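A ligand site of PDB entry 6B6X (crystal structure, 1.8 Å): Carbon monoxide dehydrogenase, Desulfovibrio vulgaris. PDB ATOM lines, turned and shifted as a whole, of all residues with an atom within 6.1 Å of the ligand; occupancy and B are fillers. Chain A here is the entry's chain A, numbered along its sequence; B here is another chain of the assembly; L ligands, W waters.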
ATOM      1  N   HIS A 105      31.963 -21.346  -9.423  1.00  0.00           N
ATOM      2  CA  HIS A 105      32.317 -20.164 -10.204  1.00  0.00           C
ATOM      3  C   HIS A 105      33.597 -19.516  -9.680  1.00  0.00           C
ATOM      4  O   HIS A 105      34.387 -18.984 -10.463  1.00  0.00           O
ATOM      5  CB  HIS A 105      31.166 -19.166 -10.189  1.00  0.00           C
ATOM      6  CG  HIS A 105      29.950 -19.627 -10.932  1.00  0.00           C
ATOM      7  ND1 HIS A 105      28.663 -19.361 -10.511  1.00  0.00           N
ATOM      8  CD2 HIS A 105      29.824 -20.357 -12.072  1.00  0.00           C
ATOM      9  CE1 HIS A 105      27.808 -19.897 -11.354  1.00  0.00           C
ATOM     10  NE2 HIS A 105      28.486 -20.506 -12.310  1.00  0.00           N
ATOM     11  N   GLY A 273      32.445 -29.481 -19.908  1.00  0.00           N
ATOM     12  CA  GLY A 273      32.886 -28.786 -18.726  1.00  0.00           C
ATOM     13  C   GLY A 273      32.700 -27.290 -18.842  1.00  0.00           C
ATOM     14  O   GLY A 273      31.672 -26.832 -19.344  1.00  0.00           O
ATOM     15  N   HIS A 274      33.698 -26.512 -18.406  1.00  0.00           N
ATOM     16  CA  HIS A 274      33.454 -25.083 -18.231  1.00  0.00           C
ATOM     17  C   HIS A 274      34.579 -24.154 -18.630  1.00  0.00           C
ATOM     18  O   HIS A 274      34.291 -23.037 -19.062  1.00  0.00           O
ATOM     19  CB  HIS A 274      33.068 -24.805 -16.765  1.00  0.00           C
ATOM     20  CG  HIS A 274      31.682 -25.228 -16.451  1.00  0.00           C
ATOM     21  ND1 HIS A 274      31.317 -26.554 -16.317  1.00  0.00           N
ATOM     22  CD2 HIS A 274      30.537 -24.510 -16.311  1.00  0.00           C
ATOM     23  CE1 HIS A 274      30.025 -26.630 -16.080  1.00  0.00           C
ATOM     24  NE2 HIS A 274      29.525 -25.405 -16.083  1.00  0.00           N
ATOM     25  N   CYS A 309      27.794 -28.011 -23.208  1.00  0.00           N
ATOM     26  CA  CYS A 309      27.543 -27.248 -21.967  1.00  0.00           C
ATOM     27  C   CYS A 309      28.352 -25.946 -22.003  1.00  0.00           C
ATOM     28  O   CYS A 309      28.457 -25.309 -23.063  1.00  0.00           O
ATOM     29  CB  CYS A 309      27.822 -28.162 -20.785  1.00  0.00           C
ATOM     30  SG  CYS A 309      26.587 -29.483 -20.590  1.00  0.00           S
ATOM     31  N   CYS A 310      28.929 -25.513 -20.883  1.00  0.00           N
ATOM     32  CA  CYS A 310      29.439 -24.142 -20.810  1.00  0.00           C
ATOM     33  C   CYS A 310      30.721 -23.962 -21.592  1.00  0.00           C
ATOM     34  O   CYS A 310      30.893 -22.941 -22.282  1.00  0.00           O
ATOM     35  CB  CYS A 310      29.640 -23.742 -19.361  1.00  0.00           C
ATOM     36  SG  CYS A 310      28.133 -23.112 -18.673  1.00  0.00           S
ATOM     37  N   ASN A 326      23.367 -29.651 -24.767  1.00  0.00           N
ATOM     38  CA  ASN A 326      23.358 -29.178 -23.401  1.00  0.00           C
ATOM     39  C   ASN A 326      23.307 -30.361 -22.430  1.00  0.00           C
ATOM     40  O   ASN A 326      23.515 -31.516 -22.824  1.00  0.00           O
ATOM     41  CB  ASN A 326      22.197 -28.193 -23.195  1.00  0.00           C
ATOM     42  CG  ASN A 326      20.860 -28.726 -23.715  1.00  0.00           C
ATOM     43  OD1 ASN A 326      20.747 -29.885 -24.109  1.00  0.00           O
ATOM     44  ND2 ASN A 326      19.844 -27.864 -23.692  1.00  0.00           N
ATOM     45  N   HIS A 327      23.010 -30.050 -21.159  1.00  0.00           N
ATOM     46  CA  HIS A 327      23.170 -30.983 -20.050  1.00  0.00           C
ATOM     47  C   HIS A 327      22.642 -32.380 -20.366  1.00  0.00           C
ATOM     48  O   HIS A 327      23.391 -33.358 -20.362  1.00  0.00           O
ATOM     49  CB  HIS A 327      22.471 -30.407 -18.811  1.00  0.00           C
ATOM     50  CG  HIS A 327      22.484 -31.296 -17.613  1.00  0.00           C
ATOM     51  ND1 HIS A 327      23.538 -32.140 -17.319  1.00  0.00           N
ATOM     52  CD2 HIS A 327      21.574 -31.477 -16.621  1.00  0.00           C
ATOM     53  CE1 HIS A 327      23.270 -32.800 -16.206  1.00  0.00           C
ATOM     54  NE2 HIS A 327      22.087 -32.412 -15.761  1.00  0.00           N
ATOM     55  N   GLN A 347      32.837 -29.638 -13.494  1.00  0.00           N
ATOM     56  CA  GLN A 347      31.476 -29.163 -13.220  1.00  0.00           C
ATOM     57  C   GLN A 347      30.468 -29.650 -14.258  1.00  0.00           C
ATOM     58  O   GLN A 347      30.677 -29.480 -15.459  1.00  0.00           O
ATOM     59  CB  GLN A 347      31.421 -27.638 -13.140  1.00  0.00           C
ATOM     60  CG  GLN A 347      32.291 -27.014 -12.080  1.00  0.00           C
ATOM     61  CD  GLN A 347      32.310 -25.511 -12.181  1.00  0.00           C
ATOM     62  OE1 GLN A 347      31.427 -24.923 -12.817  1.00  0.00           O
ATOM     63  NE2 GLN A 347      33.317 -24.876 -11.590  1.00  0.00           N
ATOM     64  N   CYS A 348      29.380 -30.253 -13.770  1.00  0.00           N
ATOM     65  CA  CYS A 348      28.253 -30.760 -14.549  1.00  0.00           C
ATOM     66  C   CYS A 348      28.628 -31.916 -15.468  1.00  0.00           C
ATOM     67  O   CYS A 348      27.844 -32.252 -16.369  1.00  0.00           O
ATOM     68  CB  CYS A 348      27.585 -29.656 -15.362  1.00  0.00           C
ATOM     69  SG  CYS A 348      27.033 -28.297 -14.330  1.00  0.00           S
ATOM     70  N   VAL A 454      18.267 -18.523 -18.139  1.00  0.00           N
ATOM     71  CA  VAL A 454      19.581 -19.062 -17.816  1.00  0.00           C
ATOM     72  C   VAL A 454      19.400 -20.478 -17.277  1.00  0.00           C
ATOM     73  O   VAL A 454      18.293 -20.937 -17.026  1.00  0.00           O
ATOM     74  CB  VAL A 454      20.313 -18.170 -16.796  1.00  0.00           C
ATOM     75  CG1 VAL A 454      20.240 -16.715 -17.238  1.00  0.00           C
ATOM     76  CG2 VAL A 454      19.684 -18.308 -15.428  1.00  0.00           C
ATOM     77  N   GLY A 455      20.507 -21.185 -17.119  1.00  0.00           N
ATOM     78  CA  GLY A 455      20.460 -22.431 -16.396  1.00  0.00           C
ATOM     79  C   GLY A 455      20.221 -23.669 -17.254  1.00  0.00           C
ATOM     80  O   GLY A 455      20.383 -23.678 -18.477  1.00  0.00           O
ATOM     81  N   CYS A 456      19.778 -24.716 -16.567  1.00  0.00           N
ATOM     82  CA  CYS A 456      20.111 -26.099 -16.876  1.00  0.00           C
ATOM     83  C   CYS A 456      18.976 -26.842 -17.586  1.00  0.00           C
ATOM     84  O   CYS A 456      18.021 -26.243 -18.100  1.00  0.00           O
ATOM     85  CB  CYS A 456      20.459 -26.819 -15.569  1.00  0.00           C
ATOM     86  SG  CYS A 456      21.331 -25.837 -14.295  1.00  0.00           S
ATOM     87  N   ASN A 457      19.121 -28.161 -17.651  1.00  0.00           N
ATOM     88  CA  ASN A 457      18.041 -29.110 -17.841  1.00  0.00           C
ATOM     89  C   ASN A 457      17.856 -29.875 -16.537  1.00  0.00           C
ATOM     90  O   ASN A 457      18.738 -29.906 -15.684  1.00  0.00           O
ATOM     91  CB  ASN A 457      18.347 -30.118 -18.953  1.00  0.00           C
ATOM     92  CG  ASN A 457      18.301 -29.499 -20.335  1.00  0.00           C
ATOM     93  OD1 ASN A 457      17.509 -28.607 -20.620  1.00  0.00           O
ATOM     94  ND2 ASN A 457      19.154 -30.005 -21.216  1.00  0.00           N
ATOM     95  N   THR A 484      21.647 -17.684 -21.754  1.00  0.00           N
ATOM     96  CA  THR A 484      22.968 -18.162 -21.375  1.00  0.00           C
ATOM     97  C   THR A 484      22.889 -19.643 -21.020  1.00  0.00           C
ATOM     98  O   THR A 484      21.802 -20.218 -20.878  1.00  0.00           O
ATOM     99  CB  THR A 484      23.548 -17.409 -20.170  1.00  0.00           C
ATOM    100  OG1 THR A 484      22.712 -17.600 -19.026  1.00  0.00           O
ATOM    101  CG2 THR A 484      23.677 -15.910 -20.469  1.00  0.00           C
ATOM    102  N   GLY A 485      24.065 -20.262 -20.901  1.00  0.00           N
ATOM    103  CA  GLY A 485      24.146 -21.627 -20.404  1.00  0.00           C
ATOM    104  C   GLY A 485      23.449 -22.617 -21.311  1.00  0.00           C
ATOM    105  O   GLY A 485      23.447 -22.489 -22.535  1.00  0.00           O
ATOM    106  N   CYS A 486      22.845 -23.625 -20.697  1.00  0.00           N
ATOM    107  CA  CYS A 486      22.203 -24.690 -21.470  1.00  0.00           C
ATOM    108  C   CYS A 486      20.935 -24.223 -22.155  1.00  0.00           C
ATOM    109  O   CYS A 486      20.470 -24.890 -23.089  1.00  0.00           O
ATOM    110  CB  CYS A 486      21.932 -25.890 -20.556  1.00  0.00           C
ATOM    111  SG  CYS A 486      23.461 -26.789 -20.187  1.00  0.00           S
ATOM    112  N   VAL A 487      20.383 -23.077 -21.743  1.00  0.00           N
ATOM    113  CA  VAL A 487      19.241 -22.509 -22.470  1.00  0.00           C
ATOM    114  C   VAL A 487      19.642 -22.139 -23.896  1.00  0.00           C
ATOM    115  O   VAL A 487      18.810 -22.170 -24.808  1.00  0.00           O
ATOM    116  CB  VAL A 487      18.699 -21.291 -21.689  1.00  0.00           C
ATOM    117  CG1 VAL A 487      17.700 -20.492 -22.529  1.00  0.00           C
ATOM    118  CG2 VAL A 487      18.043 -21.754 -20.389  1.00  0.00           C
ATOM    119  N   SER A 526      28.150 -18.351 -21.542  1.00  0.00           N
ATOM    120  CA  SER A 526      28.115 -19.451 -20.585  1.00  0.00           C
ATOM    121  C   SER A 526      27.478 -18.998 -19.277  1.00  0.00           C
ATOM    122  O   SER A 526      26.978 -17.877 -19.160  1.00  0.00           O
ATOM    123  CB  SER A 526      29.531 -19.947 -20.335  1.00  0.00           C
ATOM    124  OG  SER A 526      30.273 -18.904 -19.730  1.00  0.00           O
ATOM    125  N   CYS A 527      27.514 -19.859 -18.261  1.00  0.00           N
ATOM    126  CA  CYS A 527      26.903 -19.501 -16.983  1.00  0.00           C
ATOM    127  C   CYS A 527      27.692 -18.441 -16.242  1.00  0.00           C
ATOM    128  O   CYS A 527      27.097 -17.606 -15.547  1.00  0.00           O
ATOM    129  CB  CYS A 527      26.745 -20.757 -16.121  1.00  0.00           C
ATOM    130  SG  CYS A 527      25.594 -21.878 -16.872  1.00  0.00           S
ATOM    131  N   TYR A 561      18.922 -27.296 -12.266  1.00  0.00           N
ATOM    132  CA  TYR A 561      19.259 -28.397 -11.373  1.00  0.00           C
ATOM    133  C   TYR A 561      20.391 -28.088 -10.406  1.00  0.00           C
ATOM    134  O   TYR A 561      20.387 -28.629  -9.300  1.00  0.00           O
ATOM    135  CB  TYR A 561      19.627 -29.679 -12.182  1.00  0.00           C
ATOM    136  CG  TYR A 561      21.127 -29.843 -12.373  1.00  0.00           C
ATOM    137  CD1 TYR A 561      21.911 -30.475 -11.412  1.00  0.00           C
ATOM    138  CD2 TYR A 561      21.762 -29.338 -13.507  1.00  0.00           C
ATOM    139  CE1 TYR A 561      23.270 -30.599 -11.563  1.00  0.00           C
ATOM    140  CE2 TYR A 561      23.129 -29.456 -13.668  1.00  0.00           C
ATOM    141  CZ  TYR A 561      23.876 -30.093 -12.691  1.00  0.00           C
ATOM    142  OH  TYR A 561      25.244 -30.211 -12.852  1.00  0.00           O
ATOM    143  N   SER A 562      21.371 -27.254 -10.775  1.00  0.00           N
ATOM    144  CA  SER A 562      22.652 -27.224 -10.089  1.00  0.00           C
ATOM    145  C   SER A 562      22.678 -26.210  -8.956  1.00  0.00           C
ATOM    146  O   SER A 562      21.878 -25.268  -8.892  1.00  0.00           O
ATOM    147  CB  SER A 562      23.775 -26.889 -11.077  1.00  0.00           C
ATOM    148  OG  SER A 562      23.623 -25.566 -11.579  1.00  0.00           O
ATOM    149  N   LYS A 564      25.111 -24.193  -8.823  1.00  0.00           N
ATOM    150  CA  LYS A 564      25.514 -22.992  -9.539  1.00  0.00           C
ATOM    151  C   LYS A 564      24.316 -22.180  -9.990  1.00  0.00           C
ATOM    152  O   LYS A 564      24.316 -20.938  -9.890  1.00  0.00           O
ATOM    153  CB  LYS A 564      26.387 -23.360 -10.743  1.00  0.00           C
ATOM    154  CG  LYS A 564      27.831 -23.634 -10.375  1.00  0.00           C
ATOM    155  CD  LYS A 564      28.627 -24.025 -11.597  1.00  0.00           C
ATOM    156  CE  LYS A 564      28.192 -25.380 -12.087  1.00  0.00           C
ATOM    157  NZ  LYS A 564      28.755 -25.615 -13.433  1.00  0.00           N
ATOM    158  N   ALA A 565      23.276 -22.843 -10.492  1.00  0.00           N
ATOM    159  CA  ALA A 565      22.084 -22.137 -10.934  1.00  0.00           C
ATOM    160  C   ALA A 565      21.387 -21.434  -9.776  1.00  0.00           C
ATOM    161  O   ALA A 565      20.898 -20.313  -9.920  1.00  0.00           O
ATOM    162  CB  ALA A 565      21.134 -23.094 -11.644  1.00  0.00           C
ATOM    163  N   ILE A 568      23.334 -18.261  -9.022  1.00  0.00           N
ATOM    164  CA  ILE A 568      22.995 -17.239 -10.009  1.00  0.00           C
ATOM    165  C   ILE A 568      21.656 -16.604  -9.685  1.00  0.00           C
ATOM    166  O   ILE A 568      21.506 -15.376  -9.694  1.00  0.00           O
ATOM    167  CB  ILE A 568      23.005 -17.837 -11.435  1.00  0.00           C
ATOM    168  CG1 ILE A 568      24.435 -18.204 -11.860  1.00  0.00           C
ATOM    169  CG2 ILE A 568      22.332 -16.876 -12.429  1.00  0.00           C
ATOM    170  CD1 ILE A 568      24.509 -19.248 -12.999  1.00  0.00           C
ATOM    171  N   HIS B 210      30.579 -30.212  -5.793  1.00  0.00           N
ATOM    172  CA  HIS B 210      29.492 -29.916  -6.724  1.00  0.00           C
ATOM    173  C   HIS B 210      29.300 -31.098  -7.673  1.00  0.00           C
ATOM    174  O   HIS B 210      30.233 -31.852  -7.947  1.00  0.00           O
ATOM    175  CB  HIS B 210      29.812 -28.642  -7.517  1.00  0.00           C
ATOM    176  CG  HIS B 210      28.659 -28.101  -8.325  1.00  0.00           C
ATOM    177  ND1 HIS B 210      28.214 -28.694  -9.475  1.00  0.00           N
ATOM    178  CD2 HIS B 210      27.901 -26.994  -8.148  1.00  0.00           C
ATOM    179  CE1 HIS B 210      27.207 -27.988  -9.974  1.00  0.00           C
ATOM    180  NE2 HIS B 210      26.991 -26.956  -9.177  1.00  0.00           N
HETATM  181 FE1  LIG L   1      25.707 -26.889 -15.747  1.00  0.00          FE
HETATM  182 FE2  LIG L   1      27.645 -24.477 -16.833  1.00  0.00          FE
HETATM  183 FE3  LIG L   1      23.347 -25.719 -15.586  1.00  0.00          FE
HETATM  184 FE4  LIG L   1      24.275 -26.215 -18.007  1.00  0.00          FE
HETATM  185  S1  LIG L   1      23.447 -24.226 -17.285  1.00  0.00           S
HETATM  186  S2  LIG L   1      23.719 -27.793 -16.531  1.00  0.00           S
HETATM  187  S3  LIG L   1      25.167 -25.283 -14.198  1.00  0.00           S
HETATM  188  S4  LIG L   1      26.647 -26.308 -17.830  1.00  0.00           S
HETATM  189 NI1  LIG L   1      24.997 -23.612 -15.743  1.00  0.00          NI
HETATM  190  O   HOH W   1      27.789 -23.652 -15.052  1.00  0.00           O
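The side-chain amino group (NZ) of Lys 564 lies close to a ring nitrogen (NE2) of His 274.
N of Cys 310 is in hydrogen-bond range of O of Gly 273 (3.4 Å).
N of Cys 486 lies within hydrogen-bond range of O of Gly 455 (3.3 Å).
The side-chain sulfur (SG) of Cys 456 sits close to the side-chain hydroxyl (OG) of Ser 562 (3.6 Å).
SG of Cys 456 sits close to N of Tyr 561.
The side-chain sulfur of Cys 348 sits close to the side-chain amino group of Lys 564.
N of Ala 565 is in hydrogen-bond range of OG of Ser 562, 3.0 Å away.
The side-chain sulfur (SG) of Cys 309 lies within hydrogen-bond range of the backbone NH (N) of His 327, 3.7 Å away.
A sulfur (S1) of the ligand lies close to the backbone carbonyl oxygen (O) of Gly 455.
Merely in contact with the ligand: Tyr 561 (3.4 Å), Cys 309 (3.7 Å) and His 327 (3.7 Å).
Hydrophobic or aromatic side chains that line the ligand: His 274, His 327 and Tyr 561.
A nickel atom (NI1) of the ligand is bound by the side-chain sulfur (SG) of Cys 527 (2.2 Å).
NE2 of His 274 binds FE2 of the ligand (2.2 Å).
An iron atom (FE2) of the ligand is bound by the side-chain sulfur (SG) of Cys 310 (2.3 Å).
N of Cys 486 lies close to S1 of the ligand, at 3.5 Å.
An iron atom (FE4) of the ligand is bound by the side-chain sulfur of Cys 486 (2.4 Å).
N of Cys 456 lies close to S1 of the ligand (3.8 Å).
The side-chain sulfur of Cys 456 is bound to an iron atom (FE3) of the ligand (2.4 Å).
The side-chain sulfur (SG) of Cys 348 is bound to an iron atom (FE1) of the ligand.
A sulfur (S3) of the ligand sits close to the side-chain hydroxyl of Ser 562 (3.1 Å).
The side-chain amino group of Lys 564 lies close to a sulfur (S3) of the ligand.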
